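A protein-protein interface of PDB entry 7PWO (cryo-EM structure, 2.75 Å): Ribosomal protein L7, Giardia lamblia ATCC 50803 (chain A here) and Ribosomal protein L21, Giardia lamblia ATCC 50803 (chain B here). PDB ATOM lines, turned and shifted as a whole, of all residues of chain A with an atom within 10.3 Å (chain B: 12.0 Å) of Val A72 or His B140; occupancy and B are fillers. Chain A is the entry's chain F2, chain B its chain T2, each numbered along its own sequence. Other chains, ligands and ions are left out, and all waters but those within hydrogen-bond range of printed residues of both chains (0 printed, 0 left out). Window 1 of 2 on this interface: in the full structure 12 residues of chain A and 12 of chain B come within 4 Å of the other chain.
Among the printed residues, pairs that only touch across the chains: Gln A69 with Val B141 (3.6 Å), Gln A69 with Val B142 (3.6 Å), Gln A69 with Ser B143 (3.7 Å), Leu A70 with Val B141 (3.6 Å), Leu A70 with Ile B144 (3.5 Å), Tyr A71 with Ala B139 (3.6 Å), Val A72 with Ala B139 (3.1 Å), Pro A73 with Ala B139 (3.6 Å), Asp A74 with Ala B138 (3.2 Å), Glu A75 with Pro B136 (3.5 Å) and Pro A76 with Pro B136 (3.7 Å).
The backbone NH (N) of Leu A70 sits at hydrogen-bond distance from the backbone carbonyl oxygen (O) of Val B142 (3.1 Å).
N of His B140 lies within hydrogen-bond range of O of Val A72 (3.0 Å).
NE of Arg B137 is in salt-bridge range of OE2 of Glu A75, at 3.4 Å.
OD1 of Asp A74 sits at hydrogen-bond distance from N of Ala B139 (2.8 Å).
Of chain B, only Ala B139 (3.1 Å) and His B140 (3.0 Å) come within 4 Å of Val A72.
Of the printed residues of chain A, His B140 touches Val A72 (3.0 Å).
Of the printed residues of chain B, Leu A70 touches Val B141, Val B142 and Ile B144.
Of chain B, only Ala B139 (3.6 Å) comes within 4 Å of Pro A73.
Asp A74 touches just these residues of chain B: Ala B138 and Ala B139.
Of the printed residues of chain A, Ala B138 touches Asp A74.
Ala B139 touches four residues of chain A.
Of the printed residues of chain A, Val B141 touches Gln A69 and Leu A70.
Of the printed residues of chain A, Val B142 touches Gln A69 (3.6 Å) and Leu A70 (3.1 Å).
Printed residues of chain A within 4 Å of Ile B144: Leu A70.
Printed residues of chain B within 4 Å of Gln A69: Val B141, Val B142 and Ser B143.
Asn A63 touches none of the printed residues of chain B.
The nearest residue of chain B that does not touch Val A72 is Val B142 (4.6 Å).
The nearest printed residue of chain A that does not touch His B140 is Tyr A71 (4.01 Å).
The backbone carbonyl oxygen (O) of Ala A64 sits at hydrogen-bond distance from the backbone NH (N) of Gln A69 (3.4 Å).
O of Ala B138 sits at hydrogen-bond distance from ND1 of His B140.
Of the 16 printed residues of chain A, 8 touch a printed residue of chain B.
Hydrophobic or aromatic side chains of chain A that line the printed part of chain B: Leu A70, Tyr A71 and Val A72.
Printed residues of chain B that touch a printed residue of chain A: Pro B136, Arg B137, Ala B138, Ala B139, His B140, Val B141, Val B142, Ser B143 and Ile B144.
Hydrophobic or aromatic side chains of chain B within 4 Å of the printed part of chain A: Pro B136, Ala B138, Ala B139, Val B141 and Ile B144.
Among the printed residues, 15 pairs touch across the chains.
Among the printed residues, Asp or Glu carboxylates within 4 Å of a Lys or Arg side-chain nitrogen of the other chain: Glu A75 with Arg B137.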
ATOM      1  N   SER A  56      10.843 -12.851  24.272  1.00  0.00           N
ATOM      2  CA  SER A  56      10.845 -11.405  24.472  1.00  0.00           C
ATOM      3  C   SER A  56      11.864 -10.729  23.557  1.00  0.00           C
ATOM      4  O   SER A  56      11.541  -9.778  22.827  1.00  0.00           O
ATOM      5  CB  SER A  56      11.131 -11.070  25.937  1.00  0.00           C
ATOM      6  OG  SER A  56      10.018 -11.359  26.766  1.00  0.00           O
ATOM      7  N   GLU A  57      13.096 -11.245  23.544  1.00  0.00           N
ATOM      8  CA  GLU A  57      14.134 -10.559  22.771  1.00  0.00           C
ATOM      9  C   GLU A  57      13.948 -10.784  21.273  1.00  0.00           C
ATOM     10  O   GLU A  57      14.294  -9.909  20.471  1.00  0.00           O
ATOM     11  CB  GLU A  57      15.532 -10.987  23.232  1.00  0.00           C
ATOM     12  CG  GLU A  57      15.904 -12.452  23.073  1.00  0.00           C
ATOM     13  CD  GLU A  57      16.474 -12.752  21.686  1.00  0.00           C
ATOM     14  OE1 GLU A  57      16.925 -11.794  21.012  1.00  0.00           O
ATOM     15  OE2 GLU A  57      16.474 -13.934  21.270  1.00  0.00           O
ATOM     16  N   ALA A  60      11.462  -8.235  20.259  1.00  0.00           N
ATOM     17  CA  ALA A  60      12.089  -6.915  20.270  1.00  0.00           C
ATOM     18  C   ALA A  60      12.941  -6.697  19.023  1.00  0.00           C
ATOM     19  O   ALA A  60      12.908  -5.617  18.420  1.00  0.00           O
ATOM     20  CB  ALA A  60      12.919  -6.744  21.540  1.00  0.00           C
ATOM     21  N   ARG A  61      13.692  -7.718  18.612  1.00  0.00           N
ATOM     22  CA  ARG A  61      14.495  -7.616  17.397  1.00  0.00           C
ATOM     23  C   ARG A  61      13.616  -7.478  16.161  1.00  0.00           C
ATOM     24  O   ARG A  61      13.974  -6.775  15.213  1.00  0.00           O
ATOM     25  CB  ARG A  61      15.406  -8.836  17.272  1.00  0.00           C
ATOM     26  CG  ARG A  61      16.822  -8.604  17.785  1.00  0.00           C
ATOM     27  CD  ARG A  61      17.554  -9.895  18.075  1.00  0.00           C
ATOM     28  NE  ARG A  61      17.780 -10.693  16.870  1.00  0.00           N
ATOM     29  CZ  ARG A  61      18.031 -12.000  16.869  1.00  0.00           C
ATOM     30  NH1 ARG A  61      18.079 -12.671  18.012  1.00  0.00           N
ATOM     31  NH2 ARG A  61      18.228 -12.638  15.725  1.00  0.00           N
ATOM     32  N   GLU A  62      12.461  -8.151  16.144  1.00  0.00           N
ATOM     33  CA  GLU A  62      11.572  -8.047  14.988  1.00  0.00           C
ATOM     34  C   GLU A  62      10.933  -6.663  14.898  1.00  0.00           C
ATOM     35  O   GLU A  62      10.828  -6.084  13.805  1.00  0.00           O
ATOM     36  CB  GLU A  62      10.504  -9.136  15.054  1.00  0.00           C
ATOM     37  CG  GLU A  62      11.009 -10.540  14.734  1.00  0.00           C
ATOM     38  CD  GLU A  62      11.299 -10.760  13.255  1.00  0.00           C
ATOM     39  OE1 GLU A  62      11.897 -11.804  12.918  1.00  0.00           O
ATOM     40  OE2 GLU A  62      10.943  -9.893  12.428  1.00  0.00           O
ATOM     41  N   ASN A  63      10.502  -6.116  16.037  1.00  0.00           N
ATOM     42  CA  ASN A  63      10.034  -4.735  16.063  1.00  0.00           C
ATOM     43  C   ASN A  63      11.128  -3.788  15.587  1.00  0.00           C
ATOM     44  O   ASN A  63      10.869  -2.859  14.813  1.00  0.00           O
ATOM     45  CB  ASN A  63       9.581  -4.372  17.478  1.00  0.00           C
ATOM     46  CG  ASN A  63       9.148  -2.920  17.611  1.00  0.00           C
ATOM     47  OD1 ASN A  63       9.019  -2.193  16.626  1.00  0.00           O
ATOM     48  ND2 ASN A  63       8.937  -2.486  18.847  1.00  0.00           N
ATOM     49  N   ALA A  64      12.358  -4.011  16.037  1.00  0.00           N
ATOM     50  CA  ALA A  64      13.474  -3.217  15.544  1.00  0.00           C
ATOM     51  C   ALA A  64      13.568  -3.299  14.026  1.00  0.00           C
ATOM     52  O   ALA A  64      13.623  -2.278  13.336  1.00  0.00           O
ATOM     53  CB  ALA A  64      14.767  -3.699  16.200  1.00  0.00           C
ATOM     54  N   LEU A  65      13.536  -4.515  13.489  1.00  0.00           N
ATOM     55  CA  LEU A  65      13.791  -4.704  12.067  1.00  0.00           C
ATOM     56  C   LEU A  65      12.680  -4.128  11.194  1.00  0.00           C
ATOM     57  O   LEU A  65      12.945  -3.735  10.052  1.00  0.00           O
ATOM     58  CB  LEU A  65      14.026  -6.189  11.778  1.00  0.00           C
ATOM     59  CG  LEU A  65      14.377  -6.571  10.343  1.00  0.00           C
ATOM     60  CD1 LEU A  65      15.678  -5.903   9.980  1.00  0.00           C
ATOM     61  CD2 LEU A  65      14.531  -8.071  10.215  1.00  0.00           C
ATOM     62  N   GLN A  69      15.793   0.204  12.597  1.00  0.00           N
ATOM     63  CA  GLN A  69      16.275   0.265  13.967  1.00  0.00           C
ATOM     64  C   GLN A  69      16.818  -1.091  14.382  1.00  0.00           C
ATOM     65  O   GLN A  69      16.451  -2.132  13.830  1.00  0.00           O
ATOM     66  CB  GLN A  69      15.167   0.712  14.929  1.00  0.00           C
ATOM     67  CG  GLN A  69      14.849   2.193  14.855  1.00  0.00           C
ATOM     68  CD  GLN A  69      13.908   2.658  15.949  1.00  0.00           C
ATOM     69  OE1 GLN A  69      13.024   1.919  16.391  1.00  0.00           O
ATOM     70  NE2 GLN A  69      14.090   3.899  16.389  1.00  0.00           N
ATOM     71  N   LEU A  70      17.708  -1.067  15.367  1.00  0.00           N
ATOM     72  CA  LEU A  70      18.245  -2.282  15.951  1.00  0.00           C
ATOM     73  C   LEU A  70      17.777  -2.414  17.391  1.00  0.00           C
ATOM     74  O   LEU A  70      17.322  -1.455  18.016  1.00  0.00           O
ATOM     75  CB  LEU A  70      19.776  -2.305  15.908  1.00  0.00           C
ATOM     76  CG  LEU A  70      20.462  -2.359  14.542  1.00  0.00           C
ATOM     77  CD1 LEU A  70      21.927  -1.925  14.632  1.00  0.00           C
ATOM     78  CD2 LEU A  70      20.330  -3.718  13.889  1.00  0.00           C
ATOM     79  N   TYR A  71      17.878  -3.630  17.903  1.00  0.00           N
ATOM     80  CA  TYR A  71      17.733  -3.904  19.320  1.00  0.00           C
ATOM     81  C   TYR A  71      19.117  -4.168  19.885  1.00  0.00           C
ATOM     82  O   TYR A  71      19.864  -4.991  19.346  1.00  0.00           O
ATOM     83  CB  TYR A  71      16.825  -5.109  19.563  1.00  0.00           C
ATOM     84  CG  TYR A  71      16.530  -5.395  21.022  1.00  0.00           C
ATOM     85  CD1 TYR A  71      15.765  -4.523  21.781  1.00  0.00           C
ATOM     86  CD2 TYR A  71      17.047  -6.518  21.642  1.00  0.00           C
ATOM     87  CE1 TYR A  71      15.500  -4.780  23.110  1.00  0.00           C
ATOM     88  CE2 TYR A  71      16.798  -6.780  22.965  1.00  0.00           C
ATOM     89  CZ  TYR A  71      16.021  -5.914  23.699  1.00  0.00           C
ATOM     90  OH  TYR A  71      15.772  -6.187  25.022  1.00  0.00           O
ATOM     91  N   VAL A  72      19.472  -3.457  20.940  1.00  0.00           N
ATOM     92  CA  VAL A  72      20.695  -3.742  21.678  1.00  0.00           C
ATOM     93  C   VAL A  72      20.281  -4.357  23.010  1.00  0.00           C
ATOM     94  O   VAL A  72      19.583  -3.704  23.791  1.00  0.00           O
ATOM     95  CB  VAL A  72      21.553  -2.483  21.878  1.00  0.00           C
ATOM     96  CG1 VAL A  72      22.939  -2.864  22.329  1.00  0.00           C
ATOM     97  CG2 VAL A  72      21.630  -1.697  20.591  1.00  0.00           C
ATOM     98  N   PRO A  73      20.641  -5.603  23.286  1.00  0.00           N
ATOM     99  CA  PRO A  73      20.215  -6.243  24.538  1.00  0.00           C
ATOM    100  C   PRO A  73      21.089  -5.915  25.741  1.00  0.00           C
ATOM    101  O   PRO A  73      22.005  -5.091  25.662  1.00  0.00           O
ATOM    102  CB  PRO A  73      20.286  -7.736  24.197  1.00  0.00           C
ATOM    103  CG  PRO A  73      21.324  -7.823  23.138  1.00  0.00           C
ATOM    104  CD  PRO A  73      21.263  -6.552  22.348  1.00  0.00           C
ATOM    105  N   ASP A  74      20.794  -6.553  26.871  1.00  0.00           N
ATOM    106  CA  ASP A  74      21.571  -6.348  28.083  1.00  0.00           C
ATOM    107  C   ASP A  74      22.973  -6.933  27.938  1.00  0.00           C
ATOM    108  O   ASP A  74      23.192  -7.919  27.230  1.00  0.00           O
ATOM    109  CB  ASP A  74      20.871  -6.976  29.288  1.00  0.00           C
ATOM    110  CG  ASP A  74      19.806  -6.072  29.881  1.00  0.00           C
ATOM    111  OD1 ASP A  74      19.899  -4.838  29.697  1.00  0.00           O
ATOM    112  OD2 ASP A  74      18.866  -6.592  30.520  1.00  0.00           O
ATOM    113  N   GLU A  75      23.923  -6.302  28.617  1.00  0.00           N
ATOM    114  CA  GLU A  75      25.288  -6.795  28.699  1.00  0.00           C
ATOM    115  C   GLU A  75      25.391  -7.903  29.740  1.00  0.00           C
ATOM    116  O   GLU A  75      24.478  -8.114  30.534  1.00  0.00           O
ATOM    117  CB  GLU A  75      26.231  -5.642  29.026  1.00  0.00           C
ATOM    118  CG  GLU A  75      26.853  -5.029  27.808  1.00  0.00           C
ATOM    119  CD  GLU A  75      27.391  -3.657  28.073  1.00  0.00           C
ATOM    120  OE1 GLU A  75      27.246  -3.193  29.216  1.00  0.00           O
ATOM    121  OE2 GLU A  75      27.954  -3.044  27.144  1.00  0.00           O
ATOM    122  N   PRO A  76      26.494  -8.654  29.755  1.00  0.00           N
ATOM    123  CA  PRO A  76      26.611  -9.739  30.733  1.00  0.00           C
ATOM    124  C   PRO A  76      26.757  -9.205  32.147  1.00  0.00           C
ATOM    125  O   PRO A  76      27.560  -8.308  32.418  1.00  0.00           O
ATOM    126  CB  PRO A  76      27.871 -10.493  30.291  1.00  0.00           C
ATOM    127  CG  PRO A  76      28.201  -9.973  28.940  1.00  0.00           C
ATOM    128  CD  PRO A  76      27.670  -8.598  28.871  1.00  0.00           C
ATOM    129  N   LEU B 135      27.619  -0.188  36.570  1.00  0.00           N
ATOM    130  CA  LEU B 135      27.048  -1.448  36.143  1.00  0.00           C
ATOM    131  C   LEU B 135      27.170  -1.612  34.634  1.00  0.00           C
ATOM    132  O   LEU B 135      27.452  -0.651  33.913  1.00  0.00           O
ATOM    133  CB  LEU B 135      25.584  -1.514  36.562  1.00  0.00           C
ATOM    134  CG  LEU B 135      25.327  -1.476  38.069  1.00  0.00           C
ATOM    135  CD1 LEU B 135      24.039  -0.746  38.391  1.00  0.00           C
ATOM    136  CD2 LEU B 135      25.302  -2.883  38.619  1.00  0.00           C
ATOM    137  N   PRO B 136      26.995  -2.833  34.129  1.00  0.00           N
ATOM    138  CA  PRO B 136      26.776  -2.995  32.691  1.00  0.00           C
ATOM    139  C   PRO B 136      25.509  -2.273  32.256  1.00  0.00           C
ATOM    140  O   PRO B 136      24.522  -2.206  32.990  1.00  0.00           O
ATOM    141  CB  PRO B 136      26.661  -4.513  32.511  1.00  0.00           C
ATOM    142  CG  PRO B 136      26.453  -5.059  33.874  1.00  0.00           C
ATOM    143  CD  PRO B 136      27.115  -4.128  34.815  1.00  0.00           C
ATOM    144  N   ARG B 137      25.552  -1.730  31.047  1.00  0.00           N
ATOM    145  CA  ARG B 137      24.505  -0.860  30.537  1.00  0.00           C
ATOM    146  C   ARG B 137      23.310  -1.682  30.060  1.00  0.00           C
ATOM    147  O   ARG B 137      23.453  -2.827  29.629  1.00  0.00           O
ATOM    148  CB  ARG B 137      25.091  -0.010  29.413  1.00  0.00           C
ATOM    149  CG  ARG B 137      25.435  -0.834  28.220  1.00  0.00           C
ATOM    150  CD  ARG B 137      26.143  -0.083  27.129  1.00  0.00           C
ATOM    151  NE  ARG B 137      27.478   0.274  27.592  1.00  0.00           N
ATOM    152  CZ  ARG B 137      28.325   1.060  26.938  1.00  0.00           C
ATOM    153  NH1 ARG B 137      27.990   1.567  25.766  1.00  0.00           N
ATOM    154  NH2 ARG B 137      29.524   1.305  27.441  1.00  0.00           N
ATOM    155  N   ALA B 138      22.126  -1.079  30.128  1.00  0.00           N
ATOM    156  CA  ALA B 138      20.872  -1.772  29.871  1.00  0.00           C
ATOM    157  C   ALA B 138      20.554  -1.836  28.378  1.00  0.00           C
ATOM    158  O   ALA B 138      21.177  -1.170  27.546  1.00  0.00           O
ATOM    159  CB  ALA B 138      19.723  -1.090  30.609  1.00  0.00           C
ATOM    160  N   ALA B 139      19.543  -2.644  28.056  1.00  0.00           N
ATOM    161  CA  ALA B 139      19.068  -2.788  26.686  1.00  0.00           C
ATOM    162  C   ALA B 139      18.321  -1.540  26.225  1.00  0.00           C
ATOM    163  O   ALA B 139      17.618  -0.895  27.006  1.00  0.00           O
ATOM    164  CB  ALA B 139      18.160  -4.004  26.574  1.00  0.00           C
ATOM    165  N   HIS B 140      18.464  -1.206  24.941  1.00  0.00           N
ATOM    166  CA  HIS B 140      17.877   0.017  24.405  1.00  0.00           C
ATOM    167  C   HIS B 140      17.795  -0.085  22.886  1.00  0.00           C
ATOM    168  O   HIS B 140      18.165  -1.094  22.285  1.00  0.00           O
ATOM    169  CB  HIS B 140      18.693   1.247  24.813  1.00  0.00           C
ATOM    170  CG  HIS B 140      20.149   1.126  24.505  1.00  0.00           C
ATOM    171  ND1 HIS B 140      21.030   0.480  25.341  1.00  0.00           N
ATOM    172  CD2 HIS B 140      20.883   1.589  23.469  1.00  0.00           C
ATOM    173  CE1 HIS B 140      22.244   0.535  24.824  1.00  0.00           C
ATOM    174  NE2 HIS B 140      22.182   1.203  23.687  1.00  0.00           N
ATOM    175  N   VAL B 141      17.319   0.996  22.268  1.00  0.00           N
ATOM    176  CA  VAL B 141      17.082   1.074  20.831  1.00  0.00           C
ATOM    177  C   VAL B 141      17.915   2.196  20.236  1.00  0.00           C
ATOM    178  O   VAL B 141      17.965   3.305  20.781  1.00  0.00           O
ATOM    179  CB  VAL B 141      15.594   1.290  20.512  1.00  0.00           C
ATOM    180  CG1 VAL B 141      15.413   1.483  19.028  1.00  0.00           C
ATOM    181  CG2 VAL B 141      14.787   0.081  20.972  1.00  0.00           C
ATOM    182  N   VAL B 142      18.561   1.909  19.115  1.00  0.00           N
ATOM    183  CA  VAL B 142      19.235   2.920  18.316  1.00  0.00           C
ATOM    184  C   VAL B 142      18.717   2.818  16.890  1.00  0.00           C
ATOM    185  O   VAL B 142      18.590   1.715  16.351  1.00  0.00           O
ATOM    186  CB  VAL B 142      20.765   2.759  18.355  1.00  0.00           C
ATOM    187  CG1 VAL B 142      21.423   3.859  17.577  1.00  0.00           C
ATOM    188  CG2 VAL B 142      21.245   2.786  19.782  1.00  0.00           C
ATOM    189  N   SER B 143      18.391   3.961  16.297  1.00  0.00           N
ATOM    190  CA  SER B 143      18.075   4.004  14.881  1.00  0.00           C
ATOM    191  C   SER B 143      19.342   3.863  14.048  1.00  0.00           C
ATOM    192  O   SER B 143      20.425   4.297  14.446  1.00  0.00           O
ATOM    193  CB  SER B 143      17.366   5.306  14.535  1.00  0.00           C
ATOM    194  OG  SER B 143      18.304   6.327  14.248  1.00  0.00           O
ATOM    195  N   ILE B 144      19.197   3.230  12.887  1.00  0.00           N
ATOM    196  CA  ILE B 144      20.287   3.058  11.931  1.00  0.00           C
ATOM    197  C   ILE B 144      19.859   3.504  10.543  1.00  0.00           C
ATOM    198  O   ILE B 144      20.379   3.023   9.532  1.00  0.00           O
ATOM    199  CB  ILE B 144      20.785   1.605  11.921  1.00  0.00           C
ATOM    200  CG1 ILE B 144      19.652   0.662  11.489  1.00  0.00           C
ATOM    201  CG2 ILE B 144      21.390   1.246  13.260  1.00  0.00           C
ATOM    202  CD1 ILE B 144      20.076  -0.744  11.232  1.00  0.00           C
